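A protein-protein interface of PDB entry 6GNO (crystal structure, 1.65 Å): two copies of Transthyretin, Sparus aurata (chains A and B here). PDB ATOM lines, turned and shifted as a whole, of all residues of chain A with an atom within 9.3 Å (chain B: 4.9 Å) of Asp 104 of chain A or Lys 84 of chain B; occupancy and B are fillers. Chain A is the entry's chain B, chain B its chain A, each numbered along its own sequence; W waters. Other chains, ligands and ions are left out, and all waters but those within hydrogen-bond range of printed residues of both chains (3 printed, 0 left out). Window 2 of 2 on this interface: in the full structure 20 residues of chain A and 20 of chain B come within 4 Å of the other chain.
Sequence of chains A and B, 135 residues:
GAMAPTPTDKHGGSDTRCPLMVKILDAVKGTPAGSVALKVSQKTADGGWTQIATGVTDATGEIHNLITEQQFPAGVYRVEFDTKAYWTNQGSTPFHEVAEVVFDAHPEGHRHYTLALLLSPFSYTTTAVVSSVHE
OD2 of Asp 104 of chain A lies within salt-bridge range of NZ of Lys 84 of chain B (3.2 Å). The backbone carbonyl oxygen of Phe 95 of chain B sits at hydrogen-bond distance from the backbone NH of Asp 104 of chain A (3.5 Å). O of Val 102 of chain A lies within hydrogen-bond range of N of Glu 97 of chain B (2.9 Å). OE1 of Glu 97 of chain B sits close to OD1 of Asp 104 of chain A (2.4 Å).
N of Lys 84 of chain B lies close to OD1 of Asp 82 of chain B (3.5 Å). O of Lys 84 of chain B is in hydrogen-bond range of OG1 of Thr 88 of chain B, 3.0 Å away. The side-chain carboxylate (OE1) of Glu 97 of chain B is in salt-bridge range of the side-chain amino group (NZ) of Lys 84 of chain B, at 3.3 Å. The backbone carbonyl oxygen (O) of Val 76 of chain A is in hydrogen-bond range of the backbone NH (N) of Lys 43 of chain A, 2.9 Å away. The backbone NH (N) of Tyr 77 of chain A is in hydrogen-bond range of the backbone carbonyl oxygen (O) of Phe 103 of chain A, at 2.8 Å. The backbone NH (N) of His 106 of chain A is in hydrogen-bond range of the side-chain hydroxyl (OH) of Tyr 113 of chain A (2.8 Å).
OE1 of Glu 97 of chain B touches CG2 of Val 76 of chain A, at 3.8 Å. His 96 of chain B touches Val 101 of chain A (CD2 to CG1, 3.9 Å). His 96 of chain B touches Val 102 of chain A. Phe 103 of chain A touches Phe 95 of chain B. CA of Phe 103 of chain A touches N of Glu 97 of chain B (3.9 Å). Phe 95 of chain B touches Tyr 113 of chain A. Leu 115 of chain A touches Phe 95 of chain B. CZ of Phe 95 of chain B touches CB of Ala 128 of chain A (3.5 Å).
Printed residues of chain B within 4 Å of Val 102 of chain A: His 96 (3.3 Å) and Glu 97 (2.9 Å). Of the printed residues of chain B, Asp 104 of chain A touches Lys 84 (3.2 Å), Phe 95 (3.5 Å) and Glu 97 (2.4 Å). Pro 107 of chain A touches none of the printed residues of chain B. Arg 111 of chain A touches none of the printed residues of chain B. Printed residues of chain B within 4 Å of Ala 128 of chain A: Phe 95 (3.5 Å). Of the printed residues of chain A, Lys 84 of chain B touches Asp 104. No residue of chain A comes within 4 Å of Ala 85 of chain B.
Hydrophobic or aromatic side chains of chain B within 4 Å of the printed part of chain A: Phe 95 and His 96. Of the 22 printed residues of chain A, 8 touch a printed residue of chain B. Printed residues of chain A that touch a printed residue of chain B: Val 76, Val 101, Val 102, Phe 103, Asp 104, Tyr 113, Leu 115 and Ala 128.
No position is printed for both chains. Of the 12 pairs that touch across the chains among the printed residues, none has its exchanged pair printed and touching as well.
Water W2 lies within hydrogen-bond range of the backbone carbonyl oxygen of Asp 104 of chain A (2.5 Å) and the backbone carbonyl oxygen of Phe 95 of chain B (3.1 Å). Water W1 bridges OD2 of Asp 104 of chain A and O of Pro 94 of chain B. Water W3 bridges the side-chain carboxylate of Glu 97 of chain B and the side-chain amino group of Lys 43 of chain A.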
ATOM      1  N   LEU A  20      11.196   0.876   8.568  1.00  0.00           N
ATOM      2  CA  LEU A  20      10.928  -0.211   7.630  1.00  0.00           C
ATOM      3  C   LEU A  20       9.476  -0.156   7.187  1.00  0.00           C
ATOM      4  O   LEU A  20       8.566  -0.396   7.987  1.00  0.00           O
ATOM      5  CB  LEU A  20      11.247  -1.561   8.263  1.00  0.00           C
ATOM      6  CG  LEU A  20      11.063  -2.798   7.383  1.00  0.00           C
ATOM      7  CD1 LEU A  20      12.008  -2.772   6.185  1.00  0.00           C
ATOM      8  CD2 LEU A  20      11.291  -4.028   8.225  1.00  0.00           C
ATOM      9  N   LYS A  43      18.205 -12.066  11.918  1.00  0.00           N
ATOM     10  CA  LYS A  43      19.141 -13.183  12.001  1.00  0.00           C
ATOM     11  C   LYS A  43      19.932 -13.130  13.302  1.00  0.00           C
ATOM     12  O   LYS A  43      20.429 -12.075  13.701  1.00  0.00           O
ATOM     13  CB  LYS A  43      20.108 -13.178  10.814  1.00  0.00           C
ATOM     14  CG  LYS A  43      20.717 -14.511  10.549  1.00  0.00           C
ATOM     15  CD  LYS A  43      21.438 -14.574   9.205  1.00  0.00           C
ATOM     16  CE  LYS A  43      21.486 -16.016   8.728  1.00  0.00           C
ATOM     17  NZ  LYS A  43      22.148 -16.209   7.410  1.00  0.00           N
ATOM     18  N   TRP A  49      16.896 -17.452  13.245  1.00  0.00           N
ATOM     19  CA  TRP A  49      15.978 -16.353  12.980  1.00  0.00           C
ATOM     20  C   TRP A  49      15.081 -16.121  14.181  1.00  0.00           C
ATOM     21  O   TRP A  49      14.544 -17.067  14.762  1.00  0.00           O
ATOM     22  CB  TRP A  49      15.104 -16.619  11.746  1.00  0.00           C
ATOM     23  CG  TRP A  49      15.880 -16.707  10.473  1.00  0.00           C
ATOM     24  CD1 TRP A  49      16.276 -17.843   9.829  1.00  0.00           C
ATOM     25  CD2 TRP A  49      16.360 -15.614   9.689  1.00  0.00           C
ATOM     26  NE1 TRP A  49      16.974 -17.526   8.697  1.00  0.00           N
ATOM     27  CE2 TRP A  49      17.041 -16.162   8.585  1.00  0.00           C
ATOM     28  CE3 TRP A  49      16.278 -14.224   9.810  1.00  0.00           C
ATOM     29  CZ2 TRP A  49      17.631 -15.365   7.605  1.00  0.00           C
ATOM     30  CZ3 TRP A  49      16.865 -13.433   8.839  1.00  0.00           C
ATOM     31  CH2 TRP A  49      17.540 -14.005   7.758  1.00  0.00           C
ATOM     32  N   PHE A  72      15.532  -2.099  15.530  1.00  0.00           N
ATOM     33  CA  PHE A  72      16.125  -2.184  14.195  1.00  0.00           C
ATOM     34  C   PHE A  72      17.604  -1.811  14.243  1.00  0.00           C
ATOM     35  O   PHE A  72      18.038  -0.836  13.627  1.00  0.00           O
ATOM     36  CB  PHE A  72      15.346  -1.292  13.229  1.00  0.00           C
ATOM     37  CG  PHE A  72      15.636  -1.534  11.781  1.00  0.00           C
ATOM     38  CD1 PHE A  72      15.441  -2.780  11.204  1.00  0.00           C
ATOM     39  CD2 PHE A  72      16.038  -0.493  10.974  1.00  0.00           C
ATOM     40  CE1 PHE A  72      15.668  -2.958   9.854  1.00  0.00           C
ATOM     41  CE2 PHE A  72      16.251  -0.675   9.640  1.00  0.00           C
ATOM     42  CZ  PHE A  72      16.086  -1.900   9.087  1.00  0.00           C
ATOM     43  N   PRO A  73      18.414  -2.591  14.952  1.00  0.00           N
ATOM     44  CA  PRO A  73      19.865  -2.445  14.827  1.00  0.00           C
ATOM     45  C   PRO A  73      20.337  -2.948  13.470  1.00  0.00           C
ATOM     46  O   PRO A  73      19.585  -3.531  12.687  1.00  0.00           O
ATOM     47  CB  PRO A  73      20.390  -3.299  15.978  1.00  0.00           C
ATOM     48  CG  PRO A  73      19.359  -4.358  16.124  1.00  0.00           C
ATOM     49  CD  PRO A  73      18.055  -3.689  15.870  1.00  0.00           C
ATOM     50  N   ALA A  74      21.604  -2.683  13.169  1.00  0.00           N
ATOM     51  CA  ALA A  74      22.174  -3.239  11.957  1.00  0.00           C
ATOM     52  C   ALA A  74      22.131  -4.755  12.019  1.00  0.00           C
ATOM     53  O   ALA A  74      22.125  -5.349  13.094  1.00  0.00           O
ATOM     54  CB  ALA A  74      23.608  -2.771  11.772  1.00  0.00           C
ATOM     55  N   GLY A  75      22.095  -5.388  10.861  1.00  0.00           N
ATOM     56  CA  GLY A  75      22.117  -6.834  10.812  1.00  0.00           C
ATOM     57  C   GLY A  75      21.380  -7.332   9.596  1.00  0.00           C
ATOM     58  O   GLY A  75      20.980  -6.559   8.739  1.00  0.00           O
ATOM     59  N   VAL A  76      21.234  -8.645   9.535  1.00  0.00           N
ATOM     60  CA  VAL A  76      20.501  -9.292   8.456  1.00  0.00           C
ATOM     61  C   VAL A  76      19.051  -9.471   8.888  1.00  0.00           C
ATOM     62  O   VAL A  76      18.772 -10.011   9.960  1.00  0.00           O
ATOM     63  CB  VAL A  76      21.138 -10.641   8.081  1.00  0.00           C
ATOM     64  CG1 VAL A  76      20.298 -11.343   7.057  1.00  0.00           C
ATOM     65  CG2 VAL A  76      22.538 -10.440   7.525  1.00  0.00           C
ATOM     66  N   TYR A  77      18.133  -8.998   8.054  1.00  0.00           N
ATOM     67  CA  TYR A  77      16.699  -9.153   8.270  1.00  0.00           C
ATOM     68  C   TYR A  77      16.059  -9.902   7.117  1.00  0.00           C
ATOM     69  O   TYR A  77      16.577  -9.934   6.001  1.00  0.00           O
ATOM     70  CB  TYR A  77      16.003  -7.806   8.413  1.00  0.00           C
ATOM     71  CG  TYR A  77      16.382  -7.091   9.668  1.00  0.00           C
ATOM     72  CD1 TYR A  77      17.581  -6.395   9.752  1.00  0.00           C
ATOM     73  CD2 TYR A  77      15.543  -7.098  10.775  1.00  0.00           C
ATOM     74  CE1 TYR A  77      17.947  -5.743  10.928  1.00  0.00           C
ATOM     75  CE2 TYR A  77      15.901  -6.456  11.937  1.00  0.00           C
ATOM     76  CZ  TYR A  77      17.098  -5.777  12.010  1.00  0.00           C
ATOM     77  OH  TYR A  77      17.416  -5.137  13.193  1.00  0.00           O
ATOM     78  N   ARG A  78      14.907 -10.481   7.412  1.00  0.00           N
ATOM     79  CA  ARG A  78      14.098 -11.199   6.441  1.00  0.00           C
ATOM     80  C   ARG A  78      12.647 -10.767   6.591  1.00  0.00           C
ATOM     81  O   ARG A  78      12.111 -10.768   7.694  1.00  0.00           O
ATOM     82  CB  ARG A  78      14.245 -12.702   6.671  1.00  0.00           C
ATOM     83  CG  ARG A  78      13.310 -13.573   5.928  1.00  0.00           C
ATOM     84  CD  ARG A  78      13.628 -14.999   6.265  1.00  0.00           C
ATOM     85  NE  ARG A  78      12.958 -15.471   7.465  1.00  0.00           N
ATOM     86  CZ  ARG A  78      13.095 -16.706   7.919  1.00  0.00           C
ATOM     87  NH1 ARG A  78      13.892 -17.553   7.275  1.00  0.00           N
ATOM     88  NH2 ARG A  78      12.447 -17.101   9.000  1.00  0.00           N
ATOM     89  N   VAL A 101      12.271 -11.617   1.352  1.00  0.00           N
ATOM     90  CA  VAL A 101      13.215 -10.539   1.062  1.00  0.00           C
ATOM     91  C   VAL A 101      14.221 -10.495   2.199  1.00  0.00           C
ATOM     92  O   VAL A 101      13.856 -10.233   3.349  1.00  0.00           O
ATOM     93  CB  VAL A 101      12.492  -9.198   0.864  1.00  0.00           C
ATOM     94  CG1 VAL A 101      13.487  -8.080   0.520  1.00  0.00           C
ATOM     95  CG2 VAL A 101      11.465  -9.336  -0.236  1.00  0.00           C
ATOM     96  N   VAL A 102      15.484 -10.787   1.886  1.00  0.00           N
ATOM     97  CA  VAL A 102      16.531 -10.939   2.888  1.00  0.00           C
ATOM     98  C   VAL A 102      17.569  -9.871   2.610  1.00  0.00           C
ATOM     99  O   VAL A 102      18.110  -9.815   1.499  1.00  0.00           O
ATOM    100  CB  VAL A 102      17.163 -12.344   2.844  1.00  0.00           C
ATOM    101  CG1 VAL A 102      18.171 -12.537   4.000  1.00  0.00           C
ATOM    102  CG2 VAL A 102      16.093 -13.395   2.893  1.00  0.00           C
ATOM    103  N   PHE A 103      17.841  -9.021   3.601  1.00  0.00           N
ATOM    104  CA  PHE A 103      18.675  -7.856   3.345  1.00  0.00           C
ATOM    105  C   PHE A 103      19.510  -7.483   4.558  1.00  0.00           C
ATOM    106  O   PHE A 103      19.178  -7.803   5.696  1.00  0.00           O
ATOM    107  CB  PHE A 103      17.824  -6.662   2.901  1.00  0.00           C
ATOM    108  CG  PHE A 103      16.891  -6.130   3.952  1.00  0.00           C
ATOM    109  CD1 PHE A 103      15.642  -6.694   4.151  1.00  0.00           C
ATOM    110  CD2 PHE A 103      17.259  -5.048   4.721  1.00  0.00           C
ATOM    111  CE1 PHE A 103      14.772  -6.180   5.107  1.00  0.00           C
ATOM    112  CE2 PHE A 103      16.405  -4.532   5.706  1.00  0.00           C
ATOM    113  CZ  PHE A 103      15.159  -5.093   5.895  1.00  0.00           C
ATOM    114  N   ASP A 104      20.600  -6.793   4.261  1.00  0.00           N
ATOM    115  CA  ASP A 104      21.478  -6.200   5.249  1.00  0.00           C
ATOM    116  C   ASP A 104      20.972  -4.808   5.573  1.00  0.00           C
ATOM    117  O   ASP A 104      20.696  -4.018   4.664  1.00  0.00           O
ATOM    118  CB  ASP A 104      22.890  -6.159   4.683  1.00  0.00           C
ATOM    119  CG  ASP A 104      23.285  -7.488   4.104  1.00  0.00           C
ATOM    120  OD1 ASP A 104      23.033  -8.485   4.795  1.00  0.00           O
ATOM    121  OD2 ASP A 104      23.791  -7.548   2.968  1.00  0.00           O
ATOM    122  N   ALA A 105      20.774  -4.536   6.852  1.00  0.00           N
ATOM    123  CA  ALA A 105      20.332  -3.219   7.260  1.00  0.00           C
ATOM    124  C   ALA A 105      21.493  -2.445   7.853  1.00  0.00           C
ATOM    125  O   ALA A 105      22.279  -2.991   8.627  1.00  0.00           O
ATOM    126  CB  ALA A 105      19.217  -3.326   8.284  1.00  0.00           C
ATOM    127  N   HIS A 106      21.579  -1.168   7.480  1.00  0.00           N
ATOM    128  CA  HIS A 106      22.600  -0.242   7.956  1.00  0.00           C
ATOM    129  C   HIS A 106      21.900   1.011   8.451  1.00  0.00           C
ATOM    130  O   HIS A 106      21.950   2.059   7.813  1.00  0.00           O
ATOM    131  CB  HIS A 106      23.602   0.091   6.850  1.00  0.00           C
ATOM    132  CG  HIS A 106      24.302  -1.107   6.296  1.00  0.00           C
ATOM    133  ND1 HIS A 106      25.356  -1.712   6.944  1.00  0.00           N
ATOM    134  CD2 HIS A 106      24.094  -1.826   5.162  1.00  0.00           C
ATOM    135  CE1 HIS A 106      25.777  -2.742   6.234  1.00  0.00           C
ATOM    136  NE2 HIS A 106      25.040  -2.828   5.139  1.00  0.00           N
ATOM    137  N   PRO A 107      21.253   0.933   9.611  1.00  0.00           N
ATOM    138  CA  PRO A 107      20.390   2.038  10.070  1.00  0.00           C
ATOM    139  C   PRO A 107      21.129   3.291  10.515  1.00  0.00           C
ATOM    140  O   PRO A 107      20.480   4.323  10.705  1.00  0.00           O
ATOM    141  CB  PRO A 107      19.638   1.406  11.248  1.00  0.00           C
ATOM    142  CG  PRO A 107      20.473   0.245  11.653  1.00  0.00           C
ATOM    143  CD  PRO A 107      21.088  -0.271  10.432  1.00  0.00           C
ATOM    144  N   ARG A 111      18.683   6.226   8.414  1.00  0.00           N
ATOM    145  CA  ARG A 111      18.376   5.599   7.143  1.00  0.00           C
ATOM    146  C   ARG A 111      17.121   4.732   7.269  1.00  0.00           C
ATOM    147  O   ARG A 111      17.042   3.862   8.139  1.00  0.00           O
ATOM    148  CB  ARG A 111      19.581   4.773   6.724  1.00  0.00           C
ATOM    149  CG  ARG A 111      19.443   4.064   5.410  1.00  0.00           C
ATOM    150  CD  ARG A 111      20.743   4.109   4.607  1.00  0.00           C
ATOM    151  NE  ARG A 111      21.923   3.762   5.386  1.00  0.00           N
ATOM    152  CZ  ARG A 111      23.091   4.398   5.319  1.00  0.00           C
ATOM    153  NH1 ARG A 111      23.249   5.437   4.510  1.00  0.00           N
ATOM    154  NH2 ARG A 111      24.108   4.001   6.076  1.00  0.00           N
ATOM    155  N   TYR A 113      14.120   2.269   5.143  1.00  0.00           N
ATOM    156  CA  TYR A 113      13.994   1.313   4.052  1.00  0.00           C
ATOM    157  C   TYR A 113      12.536   1.139   3.667  1.00  0.00           C
ATOM    158  O   TYR A 113      11.684   0.938   4.532  1.00  0.00           O
ATOM    159  CB  TYR A 113      14.563  -0.049   4.458  1.00  0.00           C
ATOM    160  CG  TYR A 113      16.046  -0.032   4.700  1.00  0.00           C
ATOM    161  CD1 TYR A 113      16.554   0.256   5.957  1.00  0.00           C
ATOM    162  CD2 TYR A 113      16.939  -0.306   3.684  1.00  0.00           C
ATOM    163  CE1 TYR A 113      17.918   0.292   6.188  1.00  0.00           C
ATOM    164  CE2 TYR A 113      18.306  -0.276   3.911  1.00  0.00           C
ATOM    165  CZ  TYR A 113      18.787   0.015   5.169  1.00  0.00           C
ATOM    166  OH  TYR A 113      20.151   0.052   5.408  1.00  0.00           O
ATOM    167  N   LEU A 115      10.547  -1.512   1.294  1.00  0.00           N
ATOM    168  CA  LEU A 115      10.561  -2.716   0.477  1.00  0.00           C
ATOM    169  C   LEU A 115       9.392  -2.655  -0.490  1.00  0.00           C
ATOM    170  O   LEU A 115       8.231  -2.802  -0.090  1.00  0.00           O
ATOM    171  CB  LEU A 115      10.475  -3.968   1.340  1.00  0.00           C
ATOM    172  CG  LEU A 115      11.532  -4.125   2.417  1.00  0.00           C
ATOM    173  CD1 LEU A 115      11.299  -5.441   3.110  1.00  0.00           C
ATOM    174  CD2 LEU A 115      12.929  -4.079   1.875  1.00  0.00           C
ATOM    175  N   ALA A 128      14.311  -2.082  -3.262  1.00  0.00           N
ATOM    176  CA  ALA A 128      14.361  -1.290  -2.037  1.00  0.00           C
ATOM    177  C   ALA A 128      14.553   0.182  -2.373  1.00  0.00           C
ATOM    178  O   ALA A 128      15.285   0.512  -3.297  1.00  0.00           O
ATOM    179  CB  ALA A 128      15.492  -1.775  -1.120  1.00  0.00           C
ATOM    180  N   VAL A 130      16.012   3.291  -0.309  1.00  0.00           N
ATOM    181  CA  VAL A 130      16.782   3.530   0.903  1.00  0.00           C
ATOM    182  C   VAL A 130      17.035   5.021   1.000  1.00  0.00           C
ATOM    183  O   VAL A 130      17.630   5.613   0.091  1.00  0.00           O
ATOM    184  CB  VAL A 130      18.101   2.747   0.902  1.00  0.00           C
ATOM    185  CG1 VAL A 130      18.853   2.972   2.216  1.00  0.00           C
ATOM    186  CG2 VAL A 130      17.828   1.287   0.710  1.00  0.00           C
ATOM    187  N   ASP B  82      23.525 -16.542  -4.007  1.00  0.00           N
ATOM    188  CA  ASP B  82      24.398 -15.601  -3.312  1.00  0.00           C
ATOM    189  C   ASP B  82      24.688 -14.403  -4.216  1.00  0.00           C
ATOM    190  O   ASP B  82      25.770 -14.234  -4.785  1.00  0.00           O
ATOM    191  CB  ASP B  82      25.673 -16.279  -2.831  1.00  0.00           C
ATOM    192  CG  ASP B  82      26.476 -15.374  -1.906  1.00  0.00           C
ATOM    193  OD1 ASP B  82      26.161 -14.164  -1.832  1.00  0.00           O
ATOM    194  OD2 ASP B  82      27.415 -15.865  -1.259  1.00  0.00           O
ATOM    195  N   THR B  83      23.691 -13.523  -4.289  1.00  0.00           N
ATOM    196  CA  THR B  83      23.779 -12.333  -5.114  1.00  0.00           C
ATOM    197  C   THR B  83      24.674 -11.274  -4.479  1.00  0.00           C
ATOM    198  O   THR B  83      25.273 -10.481  -5.186  1.00  0.00           O
ATOM    199  CB  THR B  83      22.379 -11.763  -5.328  1.00  0.00           C
ATOM    200  OG1 THR B  83      21.748 -11.624  -4.057  1.00  0.00           O
ATOM    201  CG2 THR B  83      21.546 -12.715  -6.167  1.00  0.00           C
ATOM    202  N   LYS B  84      24.777 -11.238  -3.151  1.00  0.00           N
ATOM    203  CA  LYS B  84      25.629 -10.245  -2.505  1.00  0.00           C
ATOM    204  C   LYS B  84      27.065 -10.346  -3.003  1.00  0.00           C
ATOM    205  O   LYS B  84      27.663  -9.353  -3.429  1.00  0.00           O
ATOM    206  CB  LYS B  84      25.579 -10.426  -0.993  1.00  0.00           C
ATOM    207  CG  LYS B  84      26.368  -9.360  -0.230  1.00  0.00           C
ATOM    208  CD  LYS B  84      26.229  -9.596   1.253  1.00  0.00           C
ATOM    209  CE  LYS B  84      26.897  -8.529   2.080  1.00  0.00           C
ATOM    210  NZ  LYS B  84      26.700  -8.798   3.531  1.00  0.00           N
ATOM    211  N   ALA B  85      27.651 -11.536  -2.927  1.00  0.00           N
ATOM    212  CA  ALA B  85      29.028 -11.688  -3.351  1.00  0.00           C
ATOM    213  C   ALA B  85      29.184 -11.390  -4.831  1.00  0.00           C
ATOM    214  O   ALA B  85      30.222 -10.844  -5.240  1.00  0.00           O
ATOM    215  CB  ALA B  85      29.539 -13.091  -3.003  1.00  0.00           C
ATOM    216  N   TYR B  86      28.154 -11.673  -5.644  1.00  0.00           N
ATOM    217  CA  TYR B  86      28.225 -11.335  -7.067  1.00  0.00           C
ATOM    218  C   TYR B  86      28.413  -9.839  -7.256  1.00  0.00           C
ATOM    219  O   TYR B  86      29.255  -9.393  -8.045  1.00  0.00           O
ATOM    220  CB  TYR B  86      26.952 -11.799  -7.798  1.00  0.00           C
ATOM    221  CG  TYR B  86      26.965 -11.407  -9.252  1.00  0.00           C
ATOM    222  CD1 TYR B  86      27.663 -12.157 -10.192  1.00  0.00           C
ATOM    223  CD2 TYR B  86      26.310 -10.275  -9.688  1.00  0.00           C
ATOM    224  CE1 TYR B  86      27.714 -11.774 -11.529  1.00  0.00           C
ATOM    225  CE2 TYR B  86      26.358  -9.895 -11.034  1.00  0.00           C
ATOM    226  CZ  TYR B  86      27.053 -10.670 -11.943  1.00  0.00           C
ATOM    227  OH  TYR B  86      27.100 -10.342 -13.265  1.00  0.00           O
ATOM    228  N   TRP B  87      27.641  -9.044  -6.519  1.00  0.00           N
ATOM    229  CA  TRP B  87      27.726  -7.601  -6.652  1.00  0.00           C
ATOM    230  C   TRP B  87      28.996  -7.039  -6.040  1.00  0.00           C
ATOM    231  O   TRP B  87      29.641  -6.164  -6.638  1.00  0.00           O
ATOM    232  CB  TRP B  87      26.505  -6.950  -6.040  1.00  0.00           C
ATOM    233  CG  TRP B  87      25.290  -7.165  -6.923  1.00  0.00           C
ATOM    234  CD1 TRP B  87      24.138  -7.784  -6.578  1.00  0.00           C
ATOM    235  CD2 TRP B  87      25.148  -6.776  -8.296  1.00  0.00           C
ATOM    236  NE1 TRP B  87      23.281  -7.812  -7.644  1.00  0.00           N
ATOM    237  CE2 TRP B  87      23.878  -7.203  -8.716  1.00  0.00           C
ATOM    238  CE3 TRP B  87      25.978  -6.110  -9.213  1.00  0.00           C
ATOM    239  CZ2 TRP B  87      23.405  -6.975 -10.001  1.00  0.00           C
ATOM    240  CZ3 TRP B  87      25.507  -5.892 -10.496  1.00  0.00           C
ATOM    241  CH2 TRP B  87      24.234  -6.330 -10.878  1.00  0.00           C
ATOM    242  N   THR B  88      29.351  -7.483  -4.829  1.00  0.00           N
ATOM    243  CA  THR B  88      30.628  -7.063  -4.253  1.00  0.00           C
ATOM    244  C   THR B  88      31.748  -7.228  -5.270  1.00  0.00           C
ATOM    245  O   THR B  88      32.536  -6.309  -5.513  1.00  0.00           O
ATOM    246  CB  THR B  88      30.943  -7.868  -2.991  1.00  0.00           C
ATOM    247  OG1 THR B  88      29.852  -7.784  -2.073  1.00  0.00           O
ATOM    248  CG2 THR B  88      32.202  -7.343  -2.320  1.00  0.00           C
ATOM    249  N   PRO B  94      25.313  -4.112  -2.682  1.00  0.00           N
ATOM    250  CA  PRO B  94      23.931  -4.531  -2.923  1.00  0.00           C
ATOM    251  C   PRO B  94      23.048  -4.387  -1.695  1.00  0.00           C
ATOM    252  O   PRO B  94      23.503  -4.287  -0.551  1.00  0.00           O
ATOM    253  CB  PRO B  94      24.090  -6.002  -3.304  1.00  0.00           C
ATOM    254  CG  PRO B  94      25.231  -6.447  -2.483  1.00  0.00           C
ATOM    255  CD  PRO B  94      26.187  -5.282  -2.456  1.00  0.00           C
ATOM    256  N   PHE B  95      21.753  -4.382  -1.964  1.00  0.00           N
ATOM    257  CA  PHE B  95      20.752  -4.411  -0.908  1.00  0.00           C
ATOM    258  C   PHE B  95      20.567  -5.809  -0.328  1.00  0.00           C
ATOM    259  O   PHE B  95      20.625  -6.001   0.895  1.00  0.00           O
ATOM    260  CB  PHE B  95      19.415  -3.900  -1.449  1.00  0.00           C
ATOM    261  CG  PHE B  95      18.304  -3.962  -0.454  1.00  0.00           C
ATOM    262  CD1 PHE B  95      18.304  -3.127   0.653  1.00  0.00           C
ATOM    263  CD2 PHE B  95      17.253  -4.838  -0.619  1.00  0.00           C
ATOM    264  CE1 PHE B  95      17.295  -3.210   1.593  1.00  0.00           C
ATOM    265  CE2 PHE B  95      16.231  -4.903   0.320  1.00  0.00           C
ATOM    266  CZ  PHE B  95      16.257  -4.085   1.411  1.00  0.00           C
ATOM    267  N   HIS B  96      20.307  -6.798  -1.174  1.00  0.00           N
ATOM    268  CA  HIS B  96      19.918  -8.107  -0.662  1.00  0.00           C
ATOM    269  C   HIS B  96      21.121  -8.936  -0.217  1.00  0.00           C
ATOM    270  O   HIS B  96      22.218  -8.842  -0.768  1.00  0.00           O
ATOM    271  CB  HIS B  96      19.144  -8.903  -1.717  1.00  0.00           C
ATOM    272  CG  HIS B  96      17.908  -8.223  -2.225  1.00  0.00           C
ATOM    273  ND1 HIS B  96      17.909  -7.427  -3.351  1.00  0.00           N
ATOM    274  CD2 HIS B  96      16.621  -8.279  -1.805  1.00  0.00           C
ATOM    275  CE1 HIS B  96      16.679  -6.991  -3.581  1.00  0.00           C
ATOM    276  NE2 HIS B  96      15.879  -7.495  -2.657  1.00  0.00           N
ATOM    277  N   GLU B  97      20.888  -9.767   0.799  1.00  0.00           N
ATOM    278  CA  GLU B  97      21.913 -10.671   1.299  1.00  0.00           C
ATOM    279  C   GLU B  97      22.018 -11.883   0.379  1.00  0.00           C
ATOM    280  O   GLU B  97      23.117 -12.345   0.071  1.00  0.00           O
ATOM    281  CB  GLU B  97      21.555 -11.055   2.738  1.00  0.00           C
ATOM    282  CG  GLU B  97      22.327 -12.206   3.360  1.00  0.00           C
ATOM    283  CD  GLU B  97      23.603 -11.816   4.044  1.00  0.00           C
ATOM    284  OE1 GLU B  97      23.976 -10.617   4.052  1.00  0.00           O
ATOM    285  OE2 GLU B  97      24.221 -12.750   4.597  1.00  0.00           O
HETATM  286  O   HOH W   1      25.038  -5.801   1.213  1.00  0.00           O
HETATM  287  O   HOH W   2      21.798  -3.664   2.482  1.00  0.00           O
HETATM  288  O   HOH W   3      24.390 -14.016   7.213  1.00  0.00           O
